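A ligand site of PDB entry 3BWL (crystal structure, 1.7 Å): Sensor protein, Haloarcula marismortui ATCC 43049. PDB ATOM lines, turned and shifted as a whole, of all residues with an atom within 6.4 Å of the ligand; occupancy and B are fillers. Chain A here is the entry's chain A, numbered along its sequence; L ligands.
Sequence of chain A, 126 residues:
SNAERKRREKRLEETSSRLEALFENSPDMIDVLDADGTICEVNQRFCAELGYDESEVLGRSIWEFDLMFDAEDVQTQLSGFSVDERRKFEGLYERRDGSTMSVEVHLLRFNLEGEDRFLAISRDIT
OD2 of Asp 66 is in hydrogen-bond range of N1 of the ligand (2.7 Å).
OD2 of Asp 31 sits close to O1 of the ligand (2.7 Å).
Merely in contact with the ligand: Leu 33, Ile 62, Phe 69, Gln 77, Leu 78, Phe 89, Tyr 93, Val 105 and Ala 120.
Hydrophobic or aromatic side chains that line the ligand: Leu 33, Ile 62, Phe 69, Leu 78, Phe 89, Tyr 93, Val 105 and Ala 120.
Of the 24 residues printed, 11 come within 4 Å of the ligand.
The nearest printed residue that does not touch the ligand is Leu 107 (4.02 Å).
The backbone NH (N) of Leu 33 sits at hydrogen-bond distance from the backbone carbonyl oxygen (O) of Phe 118 (2.8 Å).
The side-chain carboxylate of Asp 66 lies within hydrogen-bond range of the backbone NH of Leu 92.
The side-chain hydroxyl (OG) of Ser 122 sits at hydrogen-bond distance from the side-chain hydroxyl (OH) of Tyr 93 (2.7 Å).
N of Ala 120 is in hydrogen-bond range of O of Asp 31 (2.9 Å).
The backbone NH (N) of Val 105 lies within hydrogen-bond range of the backbone carbonyl oxygen (O) of Phe 89, 2.8 Å away.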
ATOM      1  N   ASP A  31      21.025  13.159  -0.121  1.00  0.00           N
ATOM      2  CA  ASP A  31      20.681  11.866  -0.669  1.00  0.00           C
ATOM      3  C   ASP A  31      21.360  11.759  -2.028  1.00  0.00           C
ATOM      4  O   ASP A  31      21.698  12.791  -2.658  1.00  0.00           O
ATOM      5  CB  ASP A  31      19.150  11.676  -0.792  1.00  0.00           C
ATOM      6  CG  ASP A  31      18.503  12.689  -1.740  1.00  0.00           C
ATOM      7  OD1 ASP A  31      18.087  13.782  -1.280  1.00  0.00           O
ATOM      8  OD2 ASP A  31      18.344  12.353  -2.951  1.00  0.00           O
ATOM      9  N   VAL A  32      21.602  10.512  -2.417  1.00  0.00           N
ATOM     10  CA  VAL A  32      22.172  10.165  -3.719  1.00  0.00           C
ATOM     11  C   VAL A  32      21.138   9.326  -4.466  1.00  0.00           C
ATOM     12  O   VAL A  32      20.617   8.340  -3.908  1.00  0.00           O
ATOM     13  CB  VAL A  32      23.514   9.352  -3.565  1.00  0.00           C
ATOM     14  CG1 VAL A  32      24.095   9.024  -4.947  1.00  0.00           C
ATOM     15  CG2 VAL A  32      24.515  10.193  -2.763  1.00  0.00           C
ATOM     16  N   LEU A  33      20.842   9.720  -5.712  1.00  0.00           N
ATOM     17  CA  LEU A  33      19.815   9.037  -6.527  1.00  0.00           C
ATOM     18  C   LEU A  33      20.458   8.435  -7.767  1.00  0.00           C
ATOM     19  O   LEU A  33      21.476   8.915  -8.249  1.00  0.00           O
ATOM     20  CB  LEU A  33      18.723  10.011  -7.017  1.00  0.00           C
ATOM     21  CG  LEU A  33      18.029  10.867  -5.964  1.00  0.00           C
ATOM     22  CD1 LEU A  33      16.967  11.712  -6.702  1.00  0.00           C
ATOM     23  CD2 LEU A  33      17.409   9.956  -4.854  1.00  0.00           C
ATOM     24  N   PHE A  46      19.412  13.282   6.723  1.00  0.00           N
ATOM     25  CA  PHE A  46      18.204  12.992   5.928  1.00  0.00           C
ATOM     26  C   PHE A  46      17.229  12.140   6.742  1.00  0.00           C
ATOM     27  O   PHE A  46      16.057  12.482   6.864  1.00  0.00           O
ATOM     28  CB  PHE A  46      18.603  12.287   4.640  1.00  0.00           C
ATOM     29  CG  PHE A  46      17.449  12.033   3.699  1.00  0.00           C
ATOM     30  CD1 PHE A  46      17.262  12.865   2.602  1.00  0.00           C
ATOM     31  CD2 PHE A  46      16.576  10.983   3.922  1.00  0.00           C
ATOM     32  CE1 PHE A  46      16.188  12.658   1.720  1.00  0.00           C
ATOM     33  CE2 PHE A  46      15.488  10.748   3.067  1.00  0.00           C
ATOM     34  CZ  PHE A  46      15.311  11.571   1.943  1.00  0.00           C
ATOM     35  N   ILE A  62      12.422   8.706  -4.793  1.00  0.00           N
ATOM     36  CA  ILE A  62      12.340  10.018  -4.120  1.00  0.00           C
ATOM     37  C   ILE A  62      10.933  10.643  -4.140  1.00  0.00           C
ATOM     38  O   ILE A  62      10.566  11.409  -3.204  1.00  0.00           O
ATOM     39  CB  ILE A  62      13.417  10.999  -4.658  1.00  0.00           C
ATOM     40  CG1 ILE A  62      13.583  12.228  -3.745  1.00  0.00           C
ATOM     41  CG2 ILE A  62      13.089  11.387  -6.136  1.00  0.00           C
ATOM     42  CD1 ILE A  62      14.169  11.932  -2.344  1.00  0.00           C
ATOM     43  N   ASP A  66       8.739  13.314  -1.489  1.00  0.00           N
ATOM     44  CA  ASP A  66       8.518  14.710  -1.863  1.00  0.00           C
ATOM     45  C   ASP A  66       7.101  14.872  -2.398  1.00  0.00           C
ATOM     46  O   ASP A  66       6.770  14.323  -3.463  1.00  0.00           O
ATOM     47  CB  ASP A  66       9.515  15.131  -2.945  1.00  0.00           C
ATOM     48  CG  ASP A  66       9.551  16.640  -3.114  1.00  0.00           C
ATOM     49  OD1 ASP A  66       8.506  17.307  -2.822  1.00  0.00           O
ATOM     50  OD2 ASP A  66      10.612  17.174  -3.518  1.00  0.00           O
ATOM     51  N   PHE A  69       6.325  16.356  -6.065  1.00  0.00           N
ATOM     52  CA  PHE A  69       6.754  15.663  -7.312  1.00  0.00           C
ATOM     53  C   PHE A  69       6.180  14.268  -7.358  1.00  0.00           C
ATOM     54  O   PHE A  69       6.435  13.448  -6.440  1.00  0.00           O
ATOM     55  CB  PHE A  69       8.297  15.524  -7.393  1.00  0.00           C
ATOM     56  CG  PHE A  69       9.015  16.822  -7.608  1.00  0.00           C
ATOM     57  CD1 PHE A  69       9.565  17.098  -8.856  1.00  0.00           C
ATOM     58  CD2 PHE A  69       9.172  17.745  -6.558  1.00  0.00           C
ATOM     59  CE1 PHE A  69      10.256  18.259  -9.083  1.00  0.00           C
ATOM     60  CE2 PHE A  69       9.856  18.952  -6.757  1.00  0.00           C
ATOM     61  CZ  PHE A  69      10.383  19.223  -8.046  1.00  0.00           C
ATOM     62  N   ASP A  73       7.063  13.657 -12.565  1.00  0.00           N
ATOM     63  CA  ASP A  73       7.772  14.911 -12.302  1.00  0.00           C
ATOM     64  C   ASP A  73       9.240  14.670 -12.046  1.00  0.00           C
ATOM     65  O   ASP A  73      10.089  15.398 -12.545  1.00  0.00           O
ATOM     66  CB  ASP A  73       7.181  15.617 -11.087  1.00  0.00           C
ATOM     67  CG  ASP A  73       5.748  16.110 -11.320  1.00  0.00           C
ATOM     68  OD1 ASP A  73       5.469  16.580 -12.438  1.00  0.00           O
ATOM     69  OD2 ASP A  73       4.950  16.078 -10.362  1.00  0.00           O
ATOM     70  N   VAL A  74       9.534  13.641 -11.248  1.00  0.00           N
ATOM     71  CA  VAL A  74      10.938  13.282 -10.945  1.00  0.00           C
ATOM     72  C   VAL A  74      11.678  12.847 -12.213  1.00  0.00           C
ATOM     73  O   VAL A  74      12.782  13.326 -12.506  1.00  0.00           O
ATOM     74  CB  VAL A  74      11.060  12.212  -9.832  1.00  0.00           C
ATOM     75  CG1 VAL A  74      12.604  11.769  -9.673  1.00  0.00           C
ATOM     76  CG2 VAL A  74      10.467  12.714  -8.508  1.00  0.00           C
ATOM     77  N   GLN A  77      12.377  15.857 -14.359  1.00  0.00           N
ATOM     78  CA  GLN A  77      13.435  16.664 -13.737  1.00  0.00           C
ATOM     79  C   GLN A  77      14.833  16.081 -14.012  1.00  0.00           C
ATOM     80  O   GLN A  77      15.729  16.807 -14.470  1.00  0.00           O
ATOM     81  CB  GLN A  77      13.215  16.756 -12.224  1.00  0.00           C
ATOM     82  CG  GLN A  77      14.170  17.707 -11.475  1.00  0.00           C
ATOM     83  CD  GLN A  77      13.833  19.164 -11.677  1.00  0.00           C
ATOM     84  OE1 GLN A  77      13.563  19.612 -12.796  1.00  0.00           O
ATOM     85  NE2 GLN A  77      13.818  19.931 -10.587  1.00  0.00           N
ATOM     86  N   LEU A  78      15.012  14.806 -13.703  1.00  0.00           N
ATOM     87  CA  LEU A  78      16.362  14.154 -13.773  1.00  0.00           C
ATOM     88  C   LEU A  78      16.868  14.030 -15.214  1.00  0.00           C
ATOM     89  O   LEU A  78      18.053  14.272 -15.481  1.00  0.00           O
ATOM     90  CB  LEU A  78      16.315  12.790 -13.110  1.00  0.00           C
ATOM     91  CG  LEU A  78      15.941  12.726 -11.628  1.00  0.00           C
ATOM     92  CD1 LEU A  78      15.904  11.262 -11.096  1.00  0.00           C
ATOM     93  CD2 LEU A  78      16.932  13.602 -10.830  1.00  0.00           C
ATOM     94  N   PHE A  89      15.740  24.053  -6.674  1.00  0.00           N
ATOM     95  CA  PHE A  89      14.290  24.073  -6.810  1.00  0.00           C
ATOM     96  C   PHE A  89      13.659  23.679  -5.488  1.00  0.00           C
ATOM     97  O   PHE A  89      14.299  23.066  -4.635  1.00  0.00           O
ATOM     98  CB  PHE A  89      13.810  23.093  -7.907  1.00  0.00           C
ATOM     99  CG  PHE A  89      14.235  21.650  -7.654  1.00  0.00           C
ATOM    100  CD1 PHE A  89      13.423  20.774  -6.939  1.00  0.00           C
ATOM    101  CD2 PHE A  89      15.451  21.170  -8.151  1.00  0.00           C
ATOM    102  CE1 PHE A  89      13.812  19.460  -6.706  1.00  0.00           C
ATOM    103  CE2 PHE A  89      15.859  19.851  -7.931  1.00  0.00           C
ATOM    104  CZ  PHE A  89      15.028  18.993  -7.207  1.00  0.00           C
ATOM    105  N   GLU A  90      12.367  23.968  -5.372  1.00  0.00           N
ATOM    106  CA  GLU A  90      11.660  23.726  -4.136  1.00  0.00           C
ATOM    107  C   GLU A  90      11.039  22.332  -4.111  1.00  0.00           C
ATOM    108  O   GLU A  90      10.544  21.848  -5.135  1.00  0.00           O
ATOM    109  CB  GLU A  90      10.598  24.830  -3.943  1.00  0.00           C
ATOM    110  CG  GLU A  90       9.628  24.598  -2.798  1.00  0.00           C
ATOM    111  CD  GLU A  90       8.494  25.649  -2.705  1.00  0.00           C
ATOM    112  OE1 GLU A  90       8.292  26.462  -3.646  1.00  0.00           O
ATOM    113  OE2 GLU A  90       7.789  25.652  -1.657  1.00  0.00           O
ATOM    114  N   GLY A  91      11.047  21.728  -2.930  1.00  0.00           N
ATOM    115  CA  GLY A  91      10.329  20.470  -2.705  1.00  0.00           C
ATOM    116  C   GLY A  91       9.630  20.541  -1.365  1.00  0.00           C
ATOM    117  O   GLY A  91       9.769  21.557  -0.663  1.00  0.00           O
ATOM    118  N   LEU A  92       8.907  19.502  -1.033  1.00  0.00           N
ATOM    119  CA  LEU A  92       8.151  19.465   0.220  1.00  0.00           C
ATOM    120  C   LEU A  92       8.154  18.046   0.775  1.00  0.00           C
ATOM    121  O   LEU A  92       7.365  17.193   0.346  1.00  0.00           O
ATOM    122  CB  LEU A  92       6.701  19.999   0.023  1.00  0.00           C
ATOM    123  CG  LEU A  92       5.832  19.971   1.276  1.00  0.00           C
ATOM    124  CD1 LEU A  92       6.197  21.153   2.211  1.00  0.00           C
ATOM    125  CD2 LEU A  92       4.335  20.095   0.833  1.00  0.00           C
ATOM    126  N   TYR A  93       9.072  17.772   1.704  1.00  0.00           N
ATOM    127  CA  TYR A  93       9.182  16.431   2.252  1.00  0.00           C
ATOM    128  C   TYR A  93       8.063  16.136   3.239  1.00  0.00           C
ATOM    129  O   TYR A  93       7.634  17.018   3.971  1.00  0.00           O
ATOM    130  CB  TYR A  93      10.521  16.239   2.979  1.00  0.00           C
ATOM    131  CG  TYR A  93      11.725  16.186   2.044  1.00  0.00           C
ATOM    132  CD1 TYR A  93      11.725  15.311   0.938  1.00  0.00           C
ATOM    133  CD2 TYR A  93      12.865  16.929   2.294  1.00  0.00           C
ATOM    134  CE1 TYR A  93      12.832  15.235   0.096  1.00  0.00           C
ATOM    135  CE2 TYR A  93      14.005  16.864   1.461  1.00  0.00           C
ATOM    136  CZ  TYR A  93      13.959  16.031   0.347  1.00  0.00           C
ATOM    137  OH  TYR A  93      15.039  15.965  -0.486  1.00  0.00           O
ATOM    138  N   VAL A 103      11.605  22.565   1.510  1.00  0.00           N
ATOM    139  CA  VAL A 103      13.049  22.559   1.307  1.00  0.00           C
ATOM    140  C   VAL A 103      13.402  23.205  -0.020  1.00  0.00           C
ATOM    141  O   VAL A 103      12.570  23.266  -0.939  1.00  0.00           O
ATOM    142  CB  VAL A 103      13.645  21.117   1.301  1.00  0.00           C
ATOM    143  CG1 VAL A 103      13.469  20.473   2.681  1.00  0.00           C
ATOM    144  CG2 VAL A 103      12.925  20.232   0.218  1.00  0.00           C
ATOM    145  N   VAL A 105      16.095  22.200  -2.704  1.00  0.00           N
ATOM    146  CA  VAL A 105      17.015  21.136  -3.085  1.00  0.00           C
ATOM    147  C   VAL A 105      18.045  21.699  -4.044  1.00  0.00           C
ATOM    148  O   VAL A 105      17.680  22.418  -5.005  1.00  0.00           O
ATOM    149  CB  VAL A 105      16.259  19.992  -3.856  1.00  0.00           C
ATOM    150  CG1 VAL A 105      17.201  18.878  -4.157  1.00  0.00           C
ATOM    151  CG2 VAL A 105      15.115  19.454  -3.036  1.00  0.00           C
ATOM    152  N   LEU A 107      20.509  20.211  -6.596  1.00  0.00           N
ATOM    153  CA  LEU A 107      20.708  18.927  -7.178  1.00  0.00           C
ATOM    154  C   LEU A 107      21.830  18.964  -8.227  1.00  0.00           C
ATOM    155  O   LEU A 107      21.915  19.906  -9.034  1.00  0.00           O
ATOM    156  CB  LEU A 107      19.402  18.480  -7.837  1.00  0.00           C
ATOM    157  CG  LEU A 107      19.317  17.103  -8.507  1.00  0.00           C
ATOM    158  CD1 LEU A 107      19.437  16.038  -7.452  1.00  0.00           C
ATOM    159  CD2 LEU A 107      17.963  16.943  -9.174  1.00  0.00           C
ATOM    160  N   PHE A 118      22.922  11.269  -9.032  1.00  0.00           N
ATOM    161  CA  PHE A 118      22.537  12.618  -8.652  1.00  0.00           C
ATOM    162  C   PHE A 118      22.802  12.785  -7.148  1.00  0.00           C
ATOM    163  O   PHE A 118      22.483  11.893  -6.355  1.00  0.00           O
ATOM    164  CB  PHE A 118      21.050  12.863  -8.895  1.00  0.00           C
ATOM    165  CG  PHE A 118      20.680  12.912 -10.349  1.00  0.00           C
ATOM    166  CD1 PHE A 118      20.533  14.140 -10.977  1.00  0.00           C
ATOM    167  CD2 PHE A 118      20.540  11.736 -11.091  1.00  0.00           C
ATOM    168  CE1 PHE A 118      20.219  14.216 -12.341  1.00  0.00           C
ATOM    169  CE2 PHE A 118      20.217  11.795 -12.509  1.00  0.00           C
ATOM    170  CZ  PHE A 118      20.053  13.037 -13.092  1.00  0.00           C
ATOM    171  N   LEU A 119      23.343  13.931  -6.781  1.00  0.00           N
ATOM    172  CA  LEU A 119      23.618  14.267  -5.382  1.00  0.00           C
ATOM    173  C   LEU A 119      22.730  15.453  -5.060  1.00  0.00           C
ATOM    174  O   LEU A 119      22.792  16.493  -5.740  1.00  0.00           O
ATOM    175  CB  LEU A 119      25.083  14.638  -5.250  1.00  0.00           C
ATOM    176  CG  LEU A 119      25.623  15.099  -3.892  1.00  0.00           C
ATOM    177  CD1 LEU A 119      25.309  14.126  -2.738  1.00  0.00           C
ATOM    178  CD2 LEU A 119      27.168  15.377  -4.035  1.00  0.00           C
ATOM    179  N   ALA A 120      21.918  15.297  -4.025  1.00  0.00           N
ATOM    180  CA  ALA A 120      20.915  16.302  -3.623  1.00  0.00           C
ATOM    181  C   ALA A 120      21.187  16.774  -2.212  1.00  0.00           C
ATOM    182  O   ALA A 120      21.259  15.984  -1.294  1.00  0.00           O
ATOM    183  CB  ALA A 120      19.505  15.745  -3.731  1.00  0.00           C
ATOM    184  N   ILE A 121      21.394  18.067  -2.071  1.00  0.00           N
ATOM    185  CA  ILE A 121      21.528  18.694  -0.760  1.00  0.00           C
ATOM    186  C   ILE A 121      20.234  19.493  -0.502  1.00  0.00           C
ATOM    187  O   ILE A 121      19.929  20.475  -1.212  1.00  0.00           O
ATOM    188  CB  ILE A 121      22.799  19.619  -0.685  1.00  0.00           C
ATOM    189  CG1 ILE A 121      24.048  18.937  -1.284  1.00  0.00           C
ATOM    190  CG2 ILE A 121      23.016  20.102   0.736  1.00  0.00           C
ATOM    191  CD1 ILE A 121      24.455  17.597  -0.703  1.00  0.00           C
ATOM    192  N   SER A 122      19.464  19.072   0.487  1.00  0.00           N
ATOM    193  CA  SER A 122      18.170  19.722   0.813  1.00  0.00           C
ATOM    194  C   SER A 122      18.295  20.601   2.053  1.00  0.00           C
ATOM    195  O   SER A 122      18.775  20.154   3.106  1.00  0.00           O
ATOM    196  CB  SER A 122      17.083  18.663   1.026  1.00  0.00           C
ATOM    197  OG  SER A 122      17.003  17.780  -0.129  1.00  0.00           O
HETATM  198  O1  LIG L   1      17.000  14.264  -4.338  1.00  0.00           O
HETATM  199  C1  LIG L   1      16.140  14.808  -3.651  1.00  0.00           C
HETATM  200  C2  LIG L   1      14.906  15.361  -4.307  1.00  0.00           C
HETATM  201  C3  LIG L   1      13.865  15.918  -3.512  1.00  0.00           C
HETATM  202  N1  LIG L   1      12.928  16.277  -4.452  1.00  0.00           N
HETATM  203  C4  LIG L   1      13.319  15.956  -5.719  1.00  0.00           C
HETATM  204  C5  LIG L   1      14.565  15.354  -5.677  1.00  0.00           C
HETATM  205  C6  LIG L   1      15.215  14.945  -6.864  1.00  0.00           C
HETATM  206  C7  LIG L   1      14.548  15.122  -8.102  1.00  0.00           C
HETATM  207  C8  LIG L   1      13.268  15.700  -8.149  1.00  0.00           C
HETATM  208  C9  LIG L   1      12.665  16.134  -6.953  1.00  0.00           C
